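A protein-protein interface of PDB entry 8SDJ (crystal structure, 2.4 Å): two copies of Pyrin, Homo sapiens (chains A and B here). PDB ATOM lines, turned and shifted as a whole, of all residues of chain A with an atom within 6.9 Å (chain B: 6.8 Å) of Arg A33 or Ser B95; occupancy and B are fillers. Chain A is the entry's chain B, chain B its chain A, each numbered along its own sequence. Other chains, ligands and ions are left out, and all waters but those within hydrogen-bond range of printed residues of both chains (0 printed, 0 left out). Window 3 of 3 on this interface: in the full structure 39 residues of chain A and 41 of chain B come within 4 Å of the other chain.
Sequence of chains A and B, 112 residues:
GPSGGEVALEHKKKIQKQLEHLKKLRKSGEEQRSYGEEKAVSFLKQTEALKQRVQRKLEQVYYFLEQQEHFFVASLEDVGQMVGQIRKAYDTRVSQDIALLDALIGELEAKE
The side-chain hydroxyl (OG) of Ser B95 is in hydrogen-bond range of the backbone carbonyl oxygen (O) of Asp B91.
The backbone carbonyl oxygen (O) of Thr B92 is in hydrogen-bond range of the side-chain hydroxyl (OG) of Ser B95, 3.3 Å away.
The guanidinium group (NH1) of Arg A26 is in salt-bridge range of the side-chain carboxylate (OE1) of Glu A30 (2.6 Å).
The side-chain hydroxyl (OG) of Ser A34 lies close to the backbone carbonyl oxygen (O) of Glu A30.
Hydrophobic or aromatic side chains of chain B that line the printed part of chain A: Val B94 and Ile B98.
Along chain A the printed residues that touch a printed residue of chain B span positions 26 to 33.
Among the printed residues, Asp or Glu carboxylates within 4 Å of a Lys or Arg side-chain nitrogen of the other chain: Arg A33 with Asp B91 (3.8 Å).
No position is printed for both chains.
The side-chain carboxylate of Asp B91 is in salt-bridge range of the guanidinium group of Arg A33 (3.8 Å).
Arg A26 touches Ile B98.
O of Gly A29 touches CG1 of Val B94 (3.3 Å).
CD1 of Ile B98 touches C of Gly A29, 3.8 Å away.
Glu A30 touches Ile B98 (N to CD1, 3.8 Å).
Val B94 touches Arg A33.
Arg A33 touches Ser B95.
Arg A33 touches Ile B98 (NE to CD1, 3.8 Å).
Of the printed residues of chain B, Arg A26 touches Ile B98.
Of the printed residues of chain B, Gly A29 touches Val B94 and Ile B98.
Of chain B, only Asp B91, Val B94, Ser B95 and Ile B98 come within 4 Å of Arg A33.
Arg B87 touches none of the printed residues of chain A.
Printed residues of chain A within 4 Å of Asp B91: Arg A33 (3.5 Å).
The nearest residue of chain B that does not touch Arg A33 is Tyr B90 (5.8 Å).
The nearest residue of chain A that does not touch Ser B95 is Gly A29 (6.2 Å).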
ATOM      1  N   ARG A  26     -12.834 -11.597  21.629  1.00  0.00           N
ATOM      2  CA  ARG A  26     -12.909 -13.040  21.817  1.00  0.00           C
ATOM      3  C   ARG A  26     -11.995 -13.487  22.959  1.00  0.00           C
ATOM      4  O   ARG A  26     -12.290 -14.468  23.653  1.00  0.00           O
ATOM      5  CB  ARG A  26     -12.434 -13.779  20.576  1.00  0.00           C
ATOM      6  CG  ARG A  26     -12.942 -15.206  20.504  1.00  0.00           C
ATOM      7  CD  ARG A  26     -11.830 -16.123  20.078  1.00  0.00           C
ATOM      8  NE  ARG A  26     -12.346 -17.453  19.790  1.00  0.00           N
ATOM      9  CZ  ARG A  26     -12.651 -18.369  20.711  1.00  0.00           C
ATOM     10  NH1 ARG A  26     -12.510 -18.088  21.996  1.00  0.00           N
ATOM     11  NH2 ARG A  26     -13.107 -19.557  20.343  1.00  0.00           N
ATOM     12  N   LYS A  27     -10.873 -12.779  23.131  1.00  0.00           N
ATOM     13  CA  LYS A  27      -9.951 -13.084  24.212  1.00  0.00           C
ATOM     14  C   LYS A  27     -10.605 -12.689  25.534  1.00  0.00           C
ATOM     15  O   LYS A  27     -10.503 -13.422  26.523  1.00  0.00           O
ATOM     16  CB  LYS A  27      -8.608 -12.365  24.010  1.00  0.00           C
ATOM     17  CG  LYS A  27      -7.517 -12.738  25.004  1.00  0.00           C
ATOM     18  CD  LYS A  27      -6.736 -14.000  24.636  1.00  0.00           C
ATOM     19  CE  LYS A  27      -5.560 -14.257  25.557  1.00  0.00           C
ATOM     20  NZ  LYS A  27      -4.828 -13.001  25.845  1.00  0.00           N
ATOM     21  N   SER A  28     -11.231 -11.505  25.532  1.00  0.00           N
ATOM     22  CA  SER A  28     -11.933 -10.946  26.676  1.00  0.00           C
ATOM     23  C   SER A  28     -13.103 -11.834  27.114  1.00  0.00           C
ATOM     24  O   SER A  28     -13.362 -11.987  28.290  1.00  0.00           O
ATOM     25  CB  SER A  28     -12.393  -9.565  26.385  1.00  0.00           C
ATOM     26  OG  SER A  28     -13.203  -9.129  27.482  1.00  0.00           O
ATOM     27  N   GLY A  29     -13.781 -12.462  26.158  1.00  0.00           N
ATOM     28  CA  GLY A  29     -14.770 -13.480  26.438  1.00  0.00           C
ATOM     29  C   GLY A  29     -14.166 -14.631  27.236  1.00  0.00           C
ATOM     30  O   GLY A  29     -14.695 -14.955  28.290  1.00  0.00           O
ATOM     31  N   GLU A  30     -13.057 -15.215  26.747  1.00  0.00           N
ATOM     32  CA  GLU A  30     -12.438 -16.388  27.362  1.00  0.00           C
ATOM     33  C   GLU A  30     -11.951 -16.054  28.773  1.00  0.00           C
ATOM     34  O   GLU A  30     -12.188 -16.814  29.710  1.00  0.00           O
ATOM     35  CB  GLU A  30     -11.238 -16.896  26.559  1.00  0.00           C
ATOM     36  CG  GLU A  30     -11.561 -17.405  25.166  1.00  0.00           C
ATOM     37  CD  GLU A  30     -10.330 -17.418  24.266  1.00  0.00           C
ATOM     38  OE1 GLU A  30     -10.455 -16.983  23.081  1.00  0.00           O
ATOM     39  OE2 GLU A  30      -9.254 -17.840  24.741  1.00  0.00           O
ATOM     40  N   GLU A  31     -11.294 -14.901  28.927  1.00  0.00           N
ATOM     41  CA  GLU A  31     -10.903 -14.415  30.242  1.00  0.00           C
ATOM     42  C   GLU A  31     -12.080 -14.373  31.221  1.00  0.00           C
ATOM     43  O   GLU A  31     -12.019 -15.005  32.279  1.00  0.00           O
ATOM     44  CB  GLU A  31     -10.051 -13.160  30.093  1.00  0.00           C
ATOM     45  CG  GLU A  31      -8.635 -13.580  29.709  1.00  0.00           C
ATOM     46  CD  GLU A  31      -7.645 -12.579  29.157  1.00  0.00           C
ATOM     47  OE1 GLU A  31      -8.006 -11.400  29.057  1.00  0.00           O
ATOM     48  OE2 GLU A  31      -6.504 -13.004  28.824  1.00  0.00           O
ATOM     49  N   GLN A  32     -13.168 -13.712  30.797  1.00  0.00           N
ATOM     50  CA  GLN A  32     -14.429 -13.588  31.521  1.00  0.00           C
ATOM     51  C   GLN A  32     -14.899 -14.976  31.958  1.00  0.00           C
ATOM     52  O   GLN A  32     -15.232 -15.192  33.126  1.00  0.00           O
ATOM     53  CB  GLN A  32     -15.464 -12.815  30.688  1.00  0.00           C
ATOM     54  CG  GLN A  32     -15.343 -11.272  30.667  1.00  0.00           C
ATOM     55  CD  GLN A  32     -16.487 -10.664  29.834  1.00  0.00           C
ATOM     56  OE1 GLN A  32     -17.658 -10.646  30.225  1.00  0.00           O
ATOM     57  NE2 GLN A  32     -16.195 -10.140  28.648  1.00  0.00           N
ATOM     58  N   ARG A  33     -14.863 -15.957  31.052  1.00  0.00           N
ATOM     59  CA  ARG A  33     -15.408 -17.267  31.394  1.00  0.00           C
ATOM     60  C   ARG A  33     -14.506 -17.904  32.438  1.00  0.00           C
ATOM     61  O   ARG A  33     -15.012 -18.526  33.373  1.00  0.00           O
ATOM     62  CB  ARG A  33     -15.441 -18.241  30.215  1.00  0.00           C
ATOM     63  CG  ARG A  33     -16.536 -17.988  29.194  1.00  0.00           C
ATOM     64  CD  ARG A  33     -16.940 -19.292  28.536  1.00  0.00           C
ATOM     65  NE  ARG A  33     -15.968 -19.824  27.599  1.00  0.00           N
ATOM     66  CZ  ARG A  33     -15.880 -21.107  27.264  1.00  0.00           C
ATOM     67  NH1 ARG A  33     -16.701 -21.997  27.811  1.00  0.00           N
ATOM     68  NH2 ARG A  33     -14.958 -21.481  26.391  1.00  0.00           N
ATOM     69  N   SER A  34     -13.184 -17.726  32.239  1.00  0.00           N
ATOM     70  CA  SER A  34     -12.162 -18.293  33.101  1.00  0.00           C
ATOM     71  C   SER A  34     -12.244 -17.671  34.491  1.00  0.00           C
ATOM     72  O   SER A  34     -12.161 -18.395  35.482  1.00  0.00           O
ATOM     73  CB  SER A  34     -10.787 -18.110  32.526  1.00  0.00           C
ATOM     74  OG  SER A  34     -10.518 -19.137  31.592  1.00  0.00           O
ATOM     75  N   TYR A  35     -12.406 -16.340  34.532  1.00  0.00           N
ATOM     76  CA  TYR A  35     -12.407 -15.624  35.795  1.00  0.00           C
ATOM     77  C   TYR A  35     -13.640 -16.044  36.595  1.00  0.00           C
ATOM     78  O   TYR A  35     -13.533 -16.419  37.756  1.00  0.00           O
ATOM     79  CB  TYR A  35     -12.321 -14.122  35.517  1.00  0.00           C
ATOM     80  CG  TYR A  35     -12.609 -13.216  36.689  1.00  0.00           C
ATOM     81  CD1 TYR A  35     -13.907 -12.931  37.083  1.00  0.00           C
ATOM     82  CD2 TYR A  35     -11.591 -12.586  37.371  1.00  0.00           C
ATOM     83  CE1 TYR A  35     -14.176 -12.080  38.144  1.00  0.00           C
ATOM     84  CE2 TYR A  35     -11.836 -11.738  38.437  1.00  0.00           C
ATOM     85  CZ  TYR A  35     -13.135 -11.478  38.821  1.00  0.00           C
ATOM     86  OH  TYR A  35     -13.384 -10.631  39.856  1.00  0.00           O
ATOM     87  N   GLY A  36     -14.806 -16.031  35.940  1.00  0.00           N
ATOM     88  CA  GLY A  36     -16.027 -16.534  36.533  1.00  0.00           C
ATOM     89  C   GLY A  36     -15.924 -17.973  37.048  1.00  0.00           C
ATOM     90  O   GLY A  36     -16.544 -18.312  38.055  1.00  0.00           O
ATOM     91  N   GLU A  37     -15.181 -18.841  36.362  1.00  0.00           N
ATOM     92  CA  GLU A  37     -14.987 -20.175  36.907  1.00  0.00           C
ATOM     93  C   GLU A  37     -14.094 -20.126  38.157  1.00  0.00           C
ATOM     94  O   GLU A  37     -14.465 -20.589  39.237  1.00  0.00           O
ATOM     95  CB  GLU A  37     -14.439 -21.145  35.857  1.00  0.00           C
ATOM     96  CG  GLU A  37     -14.642 -22.602  36.258  1.00  0.00           C
ATOM     97  CD  GLU A  37     -13.754 -23.615  35.563  1.00  0.00           C
ATOM     98  OE1 GLU A  37     -12.520 -23.388  35.515  1.00  0.00           O
ATOM     99  OE2 GLU A  37     -14.303 -24.627  35.068  1.00  0.00           O
ATOM    100  N   GLU A  38     -12.888 -19.569  38.023  1.00  0.00           N
ATOM    101  CA  GLU A  38     -11.976 -19.633  39.149  1.00  0.00           C
ATOM    102  C   GLU A  38     -12.644 -18.980  40.357  1.00  0.00           C
ATOM    103  O   GLU A  38     -12.440 -19.422  41.482  1.00  0.00           O
ATOM    104  CB  GLU A  38     -10.559 -19.184  38.771  1.00  0.00           C
ATOM    105  CG  GLU A  38     -10.281 -17.709  38.905  1.00  0.00           C
ATOM    106  CD  GLU A  38      -8.902 -17.303  38.401  1.00  0.00           C
ATOM    107  OE1 GLU A  38      -8.572 -17.674  37.250  1.00  0.00           O
ATOM    108  OE2 GLU A  38      -8.159 -16.615  39.160  1.00  0.00           O
ATOM    109  N   ARG B  87     -22.932 -18.847  37.846  1.00  0.00           N
ATOM    110  CA  ARG B  87     -21.791 -19.279  37.039  1.00  0.00           C
ATOM    111  C   ARG B  87     -22.302 -19.856  35.715  1.00  0.00           C
ATOM    112  O   ARG B  87     -21.858 -19.445  34.649  1.00  0.00           O
ATOM    113  CB  ARG B  87     -20.876 -20.276  37.766  1.00  0.00           C
ATOM    114  CG  ARG B  87     -19.612 -20.672  37.005  1.00  0.00           C
ATOM    115  CD  ARG B  87     -19.098 -22.091  37.159  1.00  0.00           C
ATOM    116  NE  ARG B  87     -19.234 -22.675  38.491  1.00  0.00           N
ATOM    117  CZ  ARG B  87     -18.673 -23.823  38.905  1.00  0.00           C
ATOM    118  NH1 ARG B  87     -18.897 -24.277  40.132  1.00  0.00           N
ATOM    119  NH2 ARG B  87     -17.895 -24.527  38.096  1.00  0.00           N
ATOM    120  N   TYR B  90     -23.839 -17.178  33.182  1.00  0.00           N
ATOM    121  CA  TYR B  90     -22.869 -16.307  32.544  1.00  0.00           C
ATOM    122  C   TYR B  90     -22.152 -17.089  31.461  1.00  0.00           C
ATOM    123  O   TYR B  90     -22.130 -16.691  30.301  1.00  0.00           O
ATOM    124  CB  TYR B  90     -21.861 -15.786  33.565  1.00  0.00           C
ATOM    125  CG  TYR B  90     -22.044 -14.338  33.932  1.00  0.00           C
ATOM    126  CD1 TYR B  90     -21.901 -13.348  32.969  1.00  0.00           C
ATOM    127  CD2 TYR B  90     -22.322 -13.963  35.239  1.00  0.00           C
ATOM    128  CE1 TYR B  90     -22.068 -12.010  33.288  1.00  0.00           C
ATOM    129  CE2 TYR B  90     -22.463 -12.627  35.576  1.00  0.00           C
ATOM    130  CZ  TYR B  90     -22.353 -11.651  34.596  1.00  0.00           C
ATOM    131  OH  TYR B  90     -22.485 -10.325  34.907  1.00  0.00           O
ATOM    132  N   ASP B  91     -21.603 -18.223  31.876  1.00  0.00           N
ATOM    133  CA  ASP B  91     -20.898 -19.144  30.999  1.00  0.00           C
ATOM    134  C   ASP B  91     -21.624 -19.394  29.675  1.00  0.00           C
ATOM    135  O   ASP B  91     -21.036 -19.262  28.597  1.00  0.00           O
ATOM    136  CB  ASP B  91     -20.597 -20.454  31.712  1.00  0.00           C
ATOM    137  CG  ASP B  91     -19.435 -21.123  31.026  1.00  0.00           C
ATOM    138  OD1 ASP B  91     -18.308 -20.749  31.362  1.00  0.00           O
ATOM    139  OD2 ASP B  91     -19.686 -21.948  30.100  1.00  0.00           O
ATOM    140  N   THR B  92     -22.886 -19.806  29.738  1.00  0.00           N
ATOM    141  CA  THR B  92     -23.645 -20.023  28.520  1.00  0.00           C
ATOM    142  C   THR B  92     -23.569 -18.750  27.685  1.00  0.00           C
ATOM    143  O   THR B  92     -23.121 -18.766  26.552  1.00  0.00           O
ATOM    144  CB  THR B  92     -25.124 -20.285  28.823  1.00  0.00           C
ATOM    145  OG1 THR B  92     -25.195 -21.311  29.807  1.00  0.00           O
ATOM    146  CG2 THR B  92     -25.915 -20.698  27.602  1.00  0.00           C
ATOM    147  N   ARG B  93     -23.975 -17.640  28.299  1.00  0.00           N
ATOM    148  CA  ARG B  93     -24.087 -16.352  27.654  1.00  0.00           C
ATOM    149  C   ARG B  93     -22.757 -15.866  27.076  1.00  0.00           C
ATOM    150  O   ARG B  93     -22.766 -15.136  26.077  1.00  0.00           O
ATOM    151  CB  ARG B  93     -24.657 -15.294  28.593  1.00  0.00           C
ATOM    152  CG  ARG B  93     -25.011 -13.982  27.894  1.00  0.00           C
ATOM    153  CD  ARG B  93     -25.651 -14.181  26.533  1.00  0.00           C
ATOM    154  NE  ARG B  93     -26.566 -13.075  26.267  1.00  0.00           N
ATOM    155  CZ  ARG B  93     -27.843 -13.041  26.628  1.00  0.00           C
ATOM    156  NH1 ARG B  93     -28.352 -14.039  27.334  1.00  0.00           N
ATOM    157  NH2 ARG B  93     -28.607 -12.028  26.248  1.00  0.00           N
ATOM    158  N   VAL B  94     -21.621 -16.185  27.704  1.00  0.00           N
ATOM    159  CA  VAL B  94     -20.367 -15.625  27.203  1.00  0.00           C
ATOM    160  C   VAL B  94     -19.813 -16.467  26.047  1.00  0.00           C
ATOM    161  O   VAL B  94     -19.408 -15.933  25.013  1.00  0.00           O
ATOM    162  CB  VAL B  94     -19.339 -15.398  28.328  1.00  0.00           C
ATOM    163  CG1 VAL B  94     -17.931 -15.388  27.755  1.00  0.00           C
ATOM    164  CG2 VAL B  94     -19.626 -14.085  29.056  1.00  0.00           C
ATOM    165  N   SER B  95     -19.825 -17.791  26.212  1.00  0.00           N
ATOM    166  CA  SER B  95     -19.327 -18.666  25.168  1.00  0.00           C
ATOM    167  C   SER B  95     -20.204 -18.535  23.923  1.00  0.00           C
ATOM    168  O   SER B  95     -19.797 -18.888  22.815  1.00  0.00           O
ATOM    169  CB  SER B  95     -19.268 -20.089  25.661  1.00  0.00           C
ATOM    170  OG  SER B  95     -20.559 -20.670  25.625  1.00  0.00           O
ATOM    171  N   GLN B  96     -21.423 -18.041  24.131  1.00  0.00           N
ATOM    172  CA  GLN B  96     -22.362 -17.795  23.061  1.00  0.00           C
ATOM    173  C   GLN B  96     -21.855 -16.586  22.272  1.00  0.00           C
ATOM    174  O   GLN B  96     -21.577 -16.695  21.083  1.00  0.00           O
ATOM    175  CB  GLN B  96     -23.716 -17.501  23.693  1.00  0.00           C
ATOM    176  CG  GLN B  96     -24.886 -18.146  22.989  1.00  0.00           C
ATOM    177  CD  GLN B  96     -26.073 -18.191  23.914  1.00  0.00           C
ATOM    178  OE1 GLN B  96     -26.646 -17.161  24.259  1.00  0.00           O
ATOM    179  NE2 GLN B  96     -26.444 -19.396  24.322  1.00  0.00           N
ATOM    180  N   ASP B  97     -21.715 -15.446  22.966  1.00  0.00           N
ATOM    181  CA  ASP B  97     -21.031 -14.262  22.486  1.00  0.00           C
ATOM    182  C   ASP B  97     -19.753 -14.665  21.761  1.00  0.00           C
ATOM    183  O   ASP B  97     -19.399 -14.077  20.734  1.00  0.00           O
ATOM    184  CB  ASP B  97     -20.541 -13.385  23.637  1.00  0.00           C
ATOM    185  CG  ASP B  97     -21.629 -12.545  24.266  1.00  0.00           C
ATOM    186  OD1 ASP B  97     -22.798 -12.857  24.003  1.00  0.00           O
ATOM    187  OD2 ASP B  97     -21.293 -11.581  25.006  1.00  0.00           O
ATOM    188  N   ILE B  98     -19.040 -15.641  22.334  1.00  0.00           N
ATOM    189  CA  ILE B  98     -17.769 -16.044  21.762  1.00  0.00           C
ATOM    190  C   ILE B  98     -18.031 -16.633  20.382  1.00  0.00           C
ATOM    191  O   ILE B  98     -17.607 -16.048  19.395  1.00  0.00           O
ATOM    192  CB  ILE B  98     -16.954 -16.992  22.673  1.00  0.00           C
ATOM    193  CG1 ILE B  98     -16.286 -16.239  23.827  1.00  0.00           C
ATOM    194  CG2 ILE B  98     -15.922 -17.749  21.854  1.00  0.00           C
ATOM    195  CD1 ILE B  98     -15.747 -17.140  24.908  1.00  0.00           C
ATOM    196  N   ALA B  99     -18.731 -17.773  20.329  1.00  0.00           N
ATOM    197  CA  ALA B  99     -18.997 -18.427  19.059  1.00  0.00           C
ATOM    198  C   ALA B  99     -19.408 -17.387  18.012  1.00  0.00           C
ATOM    199  O   ALA B  99     -19.003 -17.462  16.856  1.00  0.00           O
ATOM    200  CB  ALA B  99     -20.021 -19.518  19.239  1.00  0.00           C
ATOM    201  N   LEU B 100     -20.152 -16.362  18.438  1.00  0.00           N
ATOM    202  CA  LEU B 100     -20.607 -15.330  17.528  1.00  0.00           C
ATOM    203  C   LEU B 100     -19.439 -14.504  17.006  1.00  0.00           C
ATOM    204  O   LEU B 100     -19.522 -13.950  15.910  1.00  0.00           O
ATOM    205  CB  LEU B 100     -21.624 -14.426  18.226  1.00  0.00           C
ATOM    206  CG  LEU B 100     -22.418 -13.513  17.296  1.00  0.00           C
ATOM    207  CD1 LEU B 100     -22.799 -14.281  16.042  1.00  0.00           C
ATOM    208  CD2 LEU B 100     -23.657 -12.983  18.002  1.00  0.00           C
